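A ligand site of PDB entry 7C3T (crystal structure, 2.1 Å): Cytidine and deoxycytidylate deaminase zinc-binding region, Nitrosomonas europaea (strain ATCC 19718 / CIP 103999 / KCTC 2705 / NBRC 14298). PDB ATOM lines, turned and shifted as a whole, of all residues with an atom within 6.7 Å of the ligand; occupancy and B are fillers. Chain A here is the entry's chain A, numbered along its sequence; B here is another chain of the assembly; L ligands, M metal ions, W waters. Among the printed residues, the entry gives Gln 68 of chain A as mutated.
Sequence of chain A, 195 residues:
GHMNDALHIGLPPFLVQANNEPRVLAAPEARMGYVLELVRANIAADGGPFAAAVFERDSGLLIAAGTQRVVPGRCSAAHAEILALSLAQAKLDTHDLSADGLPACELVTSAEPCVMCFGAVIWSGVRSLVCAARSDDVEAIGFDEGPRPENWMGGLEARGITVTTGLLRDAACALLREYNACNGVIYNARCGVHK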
ATOM      1  N   GLY A  48     -21.243  -5.128  -7.349  1.00  0.00           N
ATOM      2  CA  GLY A  48     -19.785  -4.937  -7.514  1.00  0.00           C
ATOM      3  C   GLY A  48     -19.130  -6.142  -8.161  1.00  0.00           C
ATOM      4  O   GLY A  48     -19.718  -7.263  -8.208  1.00  0.00           O
ATOM      5  N   PRO A  49     -17.877  -5.964  -8.606  1.00  0.00           N
ATOM      6  CA  PRO A  49     -17.100  -6.933  -9.348  1.00  0.00           C
ATOM      7  C   PRO A  49     -16.449  -8.057  -8.456  1.00  0.00           C
ATOM      8  O   PRO A  49     -15.253  -8.304  -8.562  1.00  0.00           O
ATOM      9  CB  PRO A  49     -16.025  -6.028  -9.995  1.00  0.00           C
ATOM     10  CG  PRO A  49     -15.747  -5.051  -8.926  1.00  0.00           C
ATOM     11  CD  PRO A  49     -17.104  -4.724  -8.373  1.00  0.00           C
ATOM     12  N   PHE A  50     -17.262  -8.717  -7.609  1.00  0.00           N
ATOM     13  CA  PHE A  50     -16.803  -9.704  -6.646  1.00  0.00           C
ATOM     14  C   PHE A  50     -17.798 -10.800  -6.539  1.00  0.00           C
ATOM     15  O   PHE A  50     -19.048 -10.563  -6.479  1.00  0.00           O
ATOM     16  CB  PHE A  50     -16.642  -9.081  -5.272  1.00  0.00           C
ATOM     17  CG  PHE A  50     -15.700  -7.935  -5.266  1.00  0.00           C
ATOM     18  CD1 PHE A  50     -14.340  -8.171  -5.230  1.00  0.00           C
ATOM     19  CD2 PHE A  50     -16.156  -6.631  -5.310  1.00  0.00           C
ATOM     20  CE1 PHE A  50     -13.425  -7.100  -5.247  1.00  0.00           C
ATOM     21  CE2 PHE A  50     -15.254  -5.561  -5.309  1.00  0.00           C
ATOM     22  CZ  PHE A  50     -13.903  -5.786  -5.290  1.00  0.00           C
ATOM     23  N   ALA A  51     -17.278 -12.007  -6.521  1.00  0.00           N
ATOM     24  CA  ALA A  51     -18.090 -13.186  -6.299  1.00  0.00           C
ATOM     25  C   ALA A  51     -17.302 -14.226  -5.526  1.00  0.00           C
ATOM     26  O   ALA A  51     -16.066 -14.238  -5.558  1.00  0.00           O
ATOM     27  CB  ALA A  51     -18.553 -13.760  -7.623  1.00  0.00           C
ATOM     28  N   THR A  67     -22.338 -13.079  -4.102  1.00  0.00           N
ATOM     29  CA  THR A  67     -21.773 -11.977  -4.838  1.00  0.00           C
ATOM     30  C   THR A  67     -21.968 -10.735  -4.044  1.00  0.00           C
ATOM     31  O   THR A  67     -22.799 -10.722  -3.178  1.00  0.00           O
ATOM     32  CB  THR A  67     -22.489 -11.859  -6.216  1.00  0.00           C
ATOM     33  OG1 THR A  67     -23.884 -11.589  -6.035  1.00  0.00           O
ATOM     34  CG2 THR A  67     -22.334 -13.099  -7.023  1.00  0.00           C
ATOM     35  N   GLN A  68     -21.181  -9.689  -4.327  1.00  0.00           N
ATOM     36  CA  GLN A  68     -21.346  -8.441  -3.632  1.00  0.00           C
ATOM     37  C   GLN A  68     -22.685  -7.761  -3.937  1.00  0.00           C
ATOM     38  O   GLN A  68     -22.978  -7.388  -5.082  1.00  0.00           O
ATOM     39  CB  GLN A  68     -20.243  -7.502  -4.023  1.00  0.00           C
ATOM     40  CG  GLN A  68     -20.206  -6.313  -3.074  1.00  0.00           C
ATOM     41  CD  GLN A  68     -20.158  -4.980  -3.704  1.00  0.00           C
ATOM     42  OE1 GLN A  68     -19.118  -4.333  -3.638  1.00  0.00           O
ATOM     43  NE2 GLN A  68     -21.336  -4.502  -4.278  1.00  0.00           N
ATOM     44  N   ARG A  69     -23.465  -7.550  -2.890  1.00  0.00           N
ATOM     45  CA  ARG A  69     -24.769  -6.974  -3.010  1.00  0.00           C
ATOM     46  C   ARG A  69     -24.899  -5.703  -2.183  1.00  0.00           C
ATOM     47  O   ARG A  69     -26.031  -5.340  -1.830  1.00  0.00           O
ATOM     48  CB  ARG A  69     -25.835  -7.959  -2.577  1.00  0.00           C
ATOM     49  CG  ARG A  69     -25.921  -9.244  -3.379  1.00  0.00           C
ATOM     50  CD  ARG A  69     -25.950  -9.019  -4.860  1.00  0.00           C
ATOM     51  NE  ARG A  69     -27.106  -8.303  -5.323  1.00  0.00           N
ATOM     52  CZ  ARG A  69     -27.276  -7.848  -6.568  1.00  0.00           C
ATOM     53  NH1 ARG A  69     -26.297  -7.919  -7.494  1.00  0.00           N
ATOM     54  NH2 ARG A  69     -28.426  -7.263  -6.881  1.00  0.00           N
ATOM     55  N   VAL A  70     -23.776  -4.999  -1.968  1.00  0.00           N
ATOM     56  CA  VAL A  70     -23.729  -3.880  -1.042  1.00  0.00           C
ATOM     57  C   VAL A  70     -24.765  -2.782  -1.378  1.00  0.00           C
ATOM     58  O   VAL A  70     -25.579  -2.407  -0.508  1.00  0.00           O
ATOM     59  CB  VAL A  70     -22.276  -3.360  -0.944  1.00  0.00           C
ATOM     60  CG1 VAL A  70     -22.192  -1.926  -0.380  1.00  0.00           C
ATOM     61  CG2 VAL A  70     -21.442  -4.336  -0.119  1.00  0.00           C
ATOM     62  N   SER A  76     -23.551  -2.752   3.827  1.00  0.00           N
ATOM     63  CA  SER A  76     -22.122  -2.692   3.611  1.00  0.00           C
ATOM     64  C   SER A  76     -21.460  -4.005   3.973  1.00  0.00           C
ATOM     65  O   SER A  76     -20.315  -4.235   3.528  1.00  0.00           O
ATOM     66  CB  SER A  76     -21.496  -1.553   4.412  1.00  0.00           C
ATOM     67  OG  SER A  76     -21.808  -1.727   5.782  1.00  0.00           O
ATOM     68  N   ALA A  78     -22.541  -6.899   2.929  1.00  0.00           N
ATOM     69  CA  ALA A  78     -22.882  -7.897   1.868  1.00  0.00           C
ATOM     70  C   ALA A  78     -21.819  -8.061   0.775  1.00  0.00           C
ATOM     71  O   ALA A  78     -22.083  -7.929  -0.433  1.00  0.00           O
ATOM     72  CB  ALA A  78     -24.206  -7.519   1.222  1.00  0.00           C
ATOM     73  N   HIS A  79     -20.609  -8.316   1.209  1.00  0.00           N
ATOM     74  CA  HIS A  79     -19.522  -8.731   0.363  1.00  0.00           C
ATOM     75  C   HIS A  79     -19.761 -10.181  -0.082  1.00  0.00           C
ATOM     76  O   HIS A  79     -20.493 -10.962   0.572  1.00  0.00           O
ATOM     77  CB  HIS A  79     -18.214  -8.631   1.137  1.00  0.00           C
ATOM     78  CG  HIS A  79     -17.756  -7.242   1.361  1.00  0.00           C
ATOM     79  ND1 HIS A  79     -16.466  -6.944   1.742  1.00  0.00           N
ATOM     80  CD2 HIS A  79     -18.393  -6.060   1.261  1.00  0.00           C
ATOM     81  CE1 HIS A  79     -16.319  -5.643   1.831  1.00  0.00           C
ATOM     82  NE2 HIS A  79     -17.464  -5.078   1.525  1.00  0.00           N
ATOM     83  N   ALA A  80     -19.115 -10.539  -1.176  1.00  0.00           N
ATOM     84  CA  ALA A  80     -19.293 -11.843  -1.797  1.00  0.00           C
ATOM     85  C   ALA A  80     -19.041 -13.038  -0.791  1.00  0.00           C
ATOM     86  O   ALA A  80     -19.856 -13.957  -0.717  1.00  0.00           O
ATOM     87  CB  ALA A  80     -18.392 -11.948  -3.005  1.00  0.00           C
ATOM     88  N   GLU A  81     -17.989 -12.908   0.029  1.00  0.00           N
ATOM     89  CA  GLU A  81     -17.523 -13.885   0.971  1.00  0.00           C
ATOM     90  C   GLU A  81     -18.534 -14.119   2.098  1.00  0.00           C
ATOM     91  O   GLU A  81     -18.855 -15.261   2.412  1.00  0.00           O
ATOM     92  CB  GLU A  81     -16.125 -13.502   1.545  1.00  0.00           C
ATOM     93  CG  GLU A  81     -15.030 -13.267   0.506  1.00  0.00           C
ATOM     94  CD  GLU A  81     -14.892 -11.794   0.041  1.00  0.00           C
ATOM     95  OE1 GLU A  81     -15.886 -11.180  -0.511  1.00  0.00           O
ATOM     96  OE2 GLU A  81     -13.772 -11.240   0.269  1.00  0.00           O
ATOM     97  N   ILE A  82     -19.072 -13.022   2.634  1.00  0.00           N
ATOM     98  CA  ILE A  82     -20.128 -13.086   3.644  1.00  0.00           C
ATOM     99  C   ILE A  82     -21.343 -13.793   3.146  1.00  0.00           C
ATOM    100  O   ILE A  82     -21.889 -14.660   3.906  1.00  0.00           O
ATOM    101  CB  ILE A  82     -20.583 -11.690   4.198  1.00  0.00           C
ATOM    102  CG1 ILE A  82     -19.392 -10.913   4.736  1.00  0.00           C
ATOM    103  CG2 ILE A  82     -21.657 -11.816   5.281  1.00  0.00           C
ATOM    104  CD1 ILE A  82     -18.506 -11.655   5.671  1.00  0.00           C
ATOM    105  N   THR A 109     -12.833 -17.426  -3.994  1.00  0.00           N
ATOM    106  CA  THR A 109     -13.125 -15.969  -4.091  1.00  0.00           C
ATOM    107  C   THR A 109     -12.433 -15.279  -5.215  1.00  0.00           C
ATOM    108  O   THR A 109     -11.258 -15.491  -5.442  1.00  0.00           O
ATOM    109  CB  THR A 109     -12.618 -15.115  -2.894  1.00  0.00           C
ATOM    110  OG1 THR A 109     -11.375 -15.620  -2.317  1.00  0.00           O
ATOM    111  CG2 THR A 109     -13.657 -15.024  -1.937  1.00  0.00           C
ATOM    112  N   SER A 110     -13.146 -14.383  -5.868  1.00  0.00           N
ATOM    113  CA  SER A 110     -12.652 -13.612  -7.059  1.00  0.00           C
ATOM    114  C   SER A 110     -11.467 -12.659  -6.691  1.00  0.00           C
ATOM    115  O   SER A 110     -10.672 -12.263  -7.567  1.00  0.00           O
ATOM    116  CB  SER A 110     -13.815 -12.842  -7.685  1.00  0.00           C
ATOM    117  OG  SER A 110     -14.253 -11.768  -6.848  1.00  0.00           O
ATOM    118  N   ALA A 111     -11.341 -12.337  -5.396  1.00  0.00           N
ATOM    119  CA  ALA A 111     -10.274 -11.458  -4.918  1.00  0.00           C
ATOM    120  C   ALA A 111      -9.913 -11.755  -3.472  1.00  0.00           C
ATOM    121  O   ALA A 111     -10.737 -12.273  -2.715  1.00  0.00           O
ATOM    122  CB  ALA A 111     -10.730 -10.010  -5.038  1.00  0.00           C
ATOM    123  N   GLU A 112      -8.692 -11.378  -3.097  1.00  0.00           N
ATOM    124  CA  GLU A 112      -8.263 -11.533  -1.730  1.00  0.00           C
ATOM    125  C   GLU A 112      -9.220 -10.820  -0.777  1.00  0.00           C
ATOM    126  O   GLU A 112      -9.797  -9.760  -1.120  1.00  0.00           O
ATOM    127  CB  GLU A 112      -6.840 -11.031  -1.561  1.00  0.00           C
ATOM    128  CG  GLU A 112      -5.859 -12.015  -2.197  1.00  0.00           C
ATOM    129  CD  GLU A 112      -4.434 -11.533  -2.161  1.00  0.00           C
ATOM    130  OE1 GLU A 112      -4.210 -10.411  -1.623  1.00  0.00           O
ATOM    131  OE2 GLU A 112      -3.574 -12.280  -2.728  1.00  0.00           O
ATOM    132  N   PRO A 113      -9.447 -11.410   0.416  1.00  0.00           N
ATOM    133  CA  PRO A 113     -10.506 -10.875   1.263  1.00  0.00           C
ATOM    134  C   PRO A 113     -10.160  -9.540   1.948  1.00  0.00           C
ATOM    135  O   PRO A 113      -9.020  -9.314   2.323  1.00  0.00           O
ATOM    136  CB  PRO A 113     -10.716 -12.001   2.289  1.00  0.00           C
ATOM    137  CG  PRO A 113      -9.370 -12.637   2.383  1.00  0.00           C
ATOM    138  CD  PRO A 113      -8.929 -12.665   0.948  1.00  0.00           C
ATOM    139  N   CYS A 114     -11.148  -8.672   2.150  1.00  0.00           N
ATOM    140  CA  CYS A 114     -10.908  -7.474   2.963  1.00  0.00           C
ATOM    141  C   CYS A 114     -10.826  -7.896   4.432  1.00  0.00           C
ATOM    142  O   CYS A 114     -11.020  -9.095   4.785  1.00  0.00           O
ATOM    143  CB  CYS A 114     -12.009  -6.439   2.784  1.00  0.00           C
ATOM    144  SG  CYS A 114     -13.558  -6.893   3.602  1.00  0.00           S
ATOM    145  N   CYS A 117     -13.982  -9.701   5.772  1.00  0.00           N
ATOM    146  CA  CYS A 117     -14.148 -11.044   5.250  1.00  0.00           C
ATOM    147  C   CYS A 117     -13.069 -11.978   5.740  1.00  0.00           C
ATOM    148  O   CYS A 117     -13.338 -13.141   5.978  1.00  0.00           O
ATOM    149  CB  CYS A 117     -14.226 -11.002   3.733  1.00  0.00           C
ATOM    150  SG  CYS A 117     -15.710 -10.131   3.181  1.00  0.00           S
ATOM    151  N   VAL A 138      -7.175  -5.035  -6.527  1.00  0.00           N
ATOM    152  CA  VAL A 138      -8.471  -4.568  -6.107  1.00  0.00           C
ATOM    153  C   VAL A 138      -8.398  -3.072  -5.743  1.00  0.00           C
ATOM    154  O   VAL A 138      -9.244  -2.307  -6.148  1.00  0.00           O
ATOM    155  CB  VAL A 138      -8.973  -5.477  -4.961  1.00  0.00           C
ATOM    156  CG1 VAL A 138     -10.210  -4.930  -4.329  1.00  0.00           C
ATOM    157  CG2 VAL A 138      -9.249  -6.856  -5.540  1.00  0.00           C
ATOM    158  N   PHE A 143     -11.195  -0.013  -4.735  1.00  0.00           N
ATOM    159  CA  PHE A 143     -11.838  -0.827  -3.696  1.00  0.00           C
ATOM    160  C   PHE A 143     -10.808  -1.065  -2.592  1.00  0.00           C
ATOM    161  O   PHE A 143      -9.760  -1.585  -2.837  1.00  0.00           O
ATOM    162  CB  PHE A 143     -12.405  -2.119  -4.252  1.00  0.00           C
ATOM    163  CG  PHE A 143     -13.742  -1.951  -4.937  1.00  0.00           C
ATOM    164  CD1 PHE A 143     -14.922  -1.756  -4.185  1.00  0.00           C
ATOM    165  CD2 PHE A 143     -13.836  -2.026  -6.325  1.00  0.00           C
ATOM    166  CE1 PHE A 143     -16.179  -1.579  -4.817  1.00  0.00           C
ATOM    167  CE2 PHE A 143     -15.072  -1.873  -6.956  1.00  0.00           C
ATOM    168  CZ  PHE A 143     -16.258  -1.641  -6.203  1.00  0.00           C
ATOM    169  N   ASP A 144     -11.143  -0.662  -1.397  1.00  0.00           N
ATOM    170  CA  ASP A 144     -10.227  -0.682  -0.249  1.00  0.00           C
ATOM    171  C   ASP A 144     -10.296  -2.054   0.395  1.00  0.00           C
ATOM    172  O   ASP A 144     -11.370  -2.562   0.564  1.00  0.00           O
ATOM    173  CB  ASP A 144     -10.747   0.397   0.712  1.00  0.00           C
ATOM    174  CG  ASP A 144      -9.819   0.727   1.877  1.00  0.00           C
ATOM    175  OD1 ASP A 144      -8.668   0.273   2.084  1.00  0.00           O
ATOM    176  OD2 ASP A 144     -10.326   1.541   2.606  1.00  0.00           O
ATOM    177  N   GLU A 145      -9.161  -2.655   0.728  1.00  0.00           N
ATOM    178  CA  GLU A 145      -9.131  -3.906   1.479  1.00  0.00           C
ATOM    179  C   GLU A 145      -9.121  -3.672   2.997  1.00  0.00           C
ATOM    180  O   GLU A 145      -9.398  -4.606   3.787  1.00  0.00           O
ATOM    181  CB  GLU A 145      -7.929  -4.775   1.105  1.00  0.00           C
ATOM    182  CG  GLU A 145      -7.956  -5.285  -0.353  1.00  0.00           C
ATOM    183  CD  GLU A 145      -8.829  -6.519  -0.574  1.00  0.00           C
ATOM    184  OE1 GLU A 145      -9.974  -6.617  -0.031  1.00  0.00           O
ATOM    185  OE2 GLU A 145      -8.384  -7.425  -1.331  1.00  0.00           O
ATOM    186  N   GLY A 146      -8.844  -2.430   3.405  1.00  0.00           N
ATOM    187  CA  GLY A 146      -8.797  -2.105   4.816  1.00  0.00           C
ATOM    188  C   GLY A 146      -7.544  -2.621   5.527  1.00  0.00           C
ATOM    189  O   GLY A 146      -6.762  -3.385   4.973  1.00  0.00           O
ATOM    190  N   TRP B 123     -16.448  -0.117   7.073  1.00  0.00           N
ATOM    191  CA  TRP B 123     -17.238   0.010   5.841  1.00  0.00           C
ATOM    192  C   TRP B 123     -18.609   0.584   6.065  1.00  0.00           C
ATOM    193  O   TRP B 123     -19.232   0.964   5.132  1.00  0.00           O
ATOM    194  CB  TRP B 123     -17.441  -1.364   5.144  1.00  0.00           C
ATOM    195  CG  TRP B 123     -16.171  -2.140   4.906  1.00  0.00           C
ATOM    196  CD1 TRP B 123     -16.015  -3.494   5.077  1.00  0.00           C
ATOM    197  CD2 TRP B 123     -14.923  -1.635   4.457  1.00  0.00           C
ATOM    198  NE1 TRP B 123     -14.707  -3.862   4.755  1.00  0.00           N
ATOM    199  CE2 TRP B 123     -14.032  -2.738   4.367  1.00  0.00           C
ATOM    200  CE3 TRP B 123     -14.464  -0.360   4.121  1.00  0.00           C
ATOM    201  CZ2 TRP B 123     -12.679  -2.591   4.001  1.00  0.00           C
ATOM    202  CZ3 TRP B 123     -13.146  -0.216   3.724  1.00  0.00           C
ATOM    203  CH2 TRP B 123     -12.266  -1.340   3.668  1.00  0.00           C
HETATM  204  C1  LIG L   1     -15.119  -7.531  -1.604  1.00  0.00           C
HETATM  205  N1  LIG L   1     -13.870  -6.979  -1.316  1.00  0.00           N
HETATM  206  C2  LIG L   1     -13.711  -5.611  -1.281  1.00  0.00           C
HETATM  207  N2  LIG L   1     -12.523  -5.032  -1.007  1.00  0.00           N
HETATM  208  N3  LIG L   1     -14.724  -4.745  -1.534  1.00  0.00           N
HETATM  209  C3  LIG L   1     -15.962  -5.201  -1.842  1.00  0.00           C
HETATM  210  O1  LIG L   1     -16.879  -4.334  -2.142  1.00  0.00           O
HETATM  211  C4  LIG L   1     -16.273  -6.652  -1.901  1.00  0.00           C
HETATM  212  N4  LIG L   1     -17.335  -7.452  -2.162  1.00  0.00           N
HETATM  213  N5  LIG L   1     -17.016  -8.772  -2.058  1.00  0.00           N
HETATM  214  N6  LIG L   1     -15.566  -8.835  -1.727  1.00  0.00           N
HETATM  215 ZN    ZN M   1     -14.930  -8.210   2.305  1.00  0.00          ZN
HETATM  216  O   HOH W   1     -13.659  -8.843   0.913  1.00  0.00           O
HETATM  217  O   HOH W   2     -12.389  -8.915  -2.437  1.00  0.00           O
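OE1 of Glu 81 sits at hydrogen-bond distance from N6 of the ligand, 2.7 Å away. An oxygen (O1) of the ligand lies within hydrogen-bond range of the side-chain amide oxygen of Gln 68, 2.7 Å away. N of Ala 80 sits at hydrogen-bond distance from N5 of the ligand (2.9 Å). O of Asp 144 lies within hydrogen-bond range of N2 of the ligand, at 3.1 Å. N2 of the ligand sits at hydrogen-bond distance from OE1 of Glu 145 (3.2 Å).
The side-chain sulfur of Cys 117 sits close to the side-chain carboxylate of Glu 81, 3.7 Å away. N of Gln 68 lies within hydrogen-bond range of O of Phe 50, at 3.2 Å. The side-chain amide nitrogen (NE2) of Gln 68 lies close to the backbone NH (N) of Val 70, 3.4 Å away. The side-chain amide nitrogen of Gln 68 sits close to the backbone NH of Gly 48, at 3.1 Å. The side-chain carboxylate (OD1) of Asp 144 lies within hydrogen-bond range of the backbone NH (N) of Gly 146, 3.0 Å away. The backbone NH of Cys 114 is in hydrogen-bond range of the side-chain carboxylate of Glu 145 (3.2 Å). The side-chain carboxylate (OE2) of Glu 145 lies close to the backbone carbonyl oxygen (O) of Glu 112 (2.7 Å). The backbone NH (N) of Phe 143 sits at hydrogen-bond distance from the backbone carbonyl oxygen (O) of Val 138 (3.3 Å).
Merely in contact with the ligand: Phe 50 (3.3 Å), His 79 (3.4 Å) and Phe 143 (3.8 Å). Of the 27 residues printed, 8 come within 4 Å of the ligand. The nearest printed residue that does not touch the ligand is Val 138 (4.05 Å).
Water W2 bridges N1 of the ligand (2.7 Å) and O of Glu 112 (3.0 Å). Water W1 lies within hydrogen-bond range of OE2 of Glu 81 (2.5 Å), N of Cys 114 (2.8 Å) and N1 of the ligand (2.9 Å).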
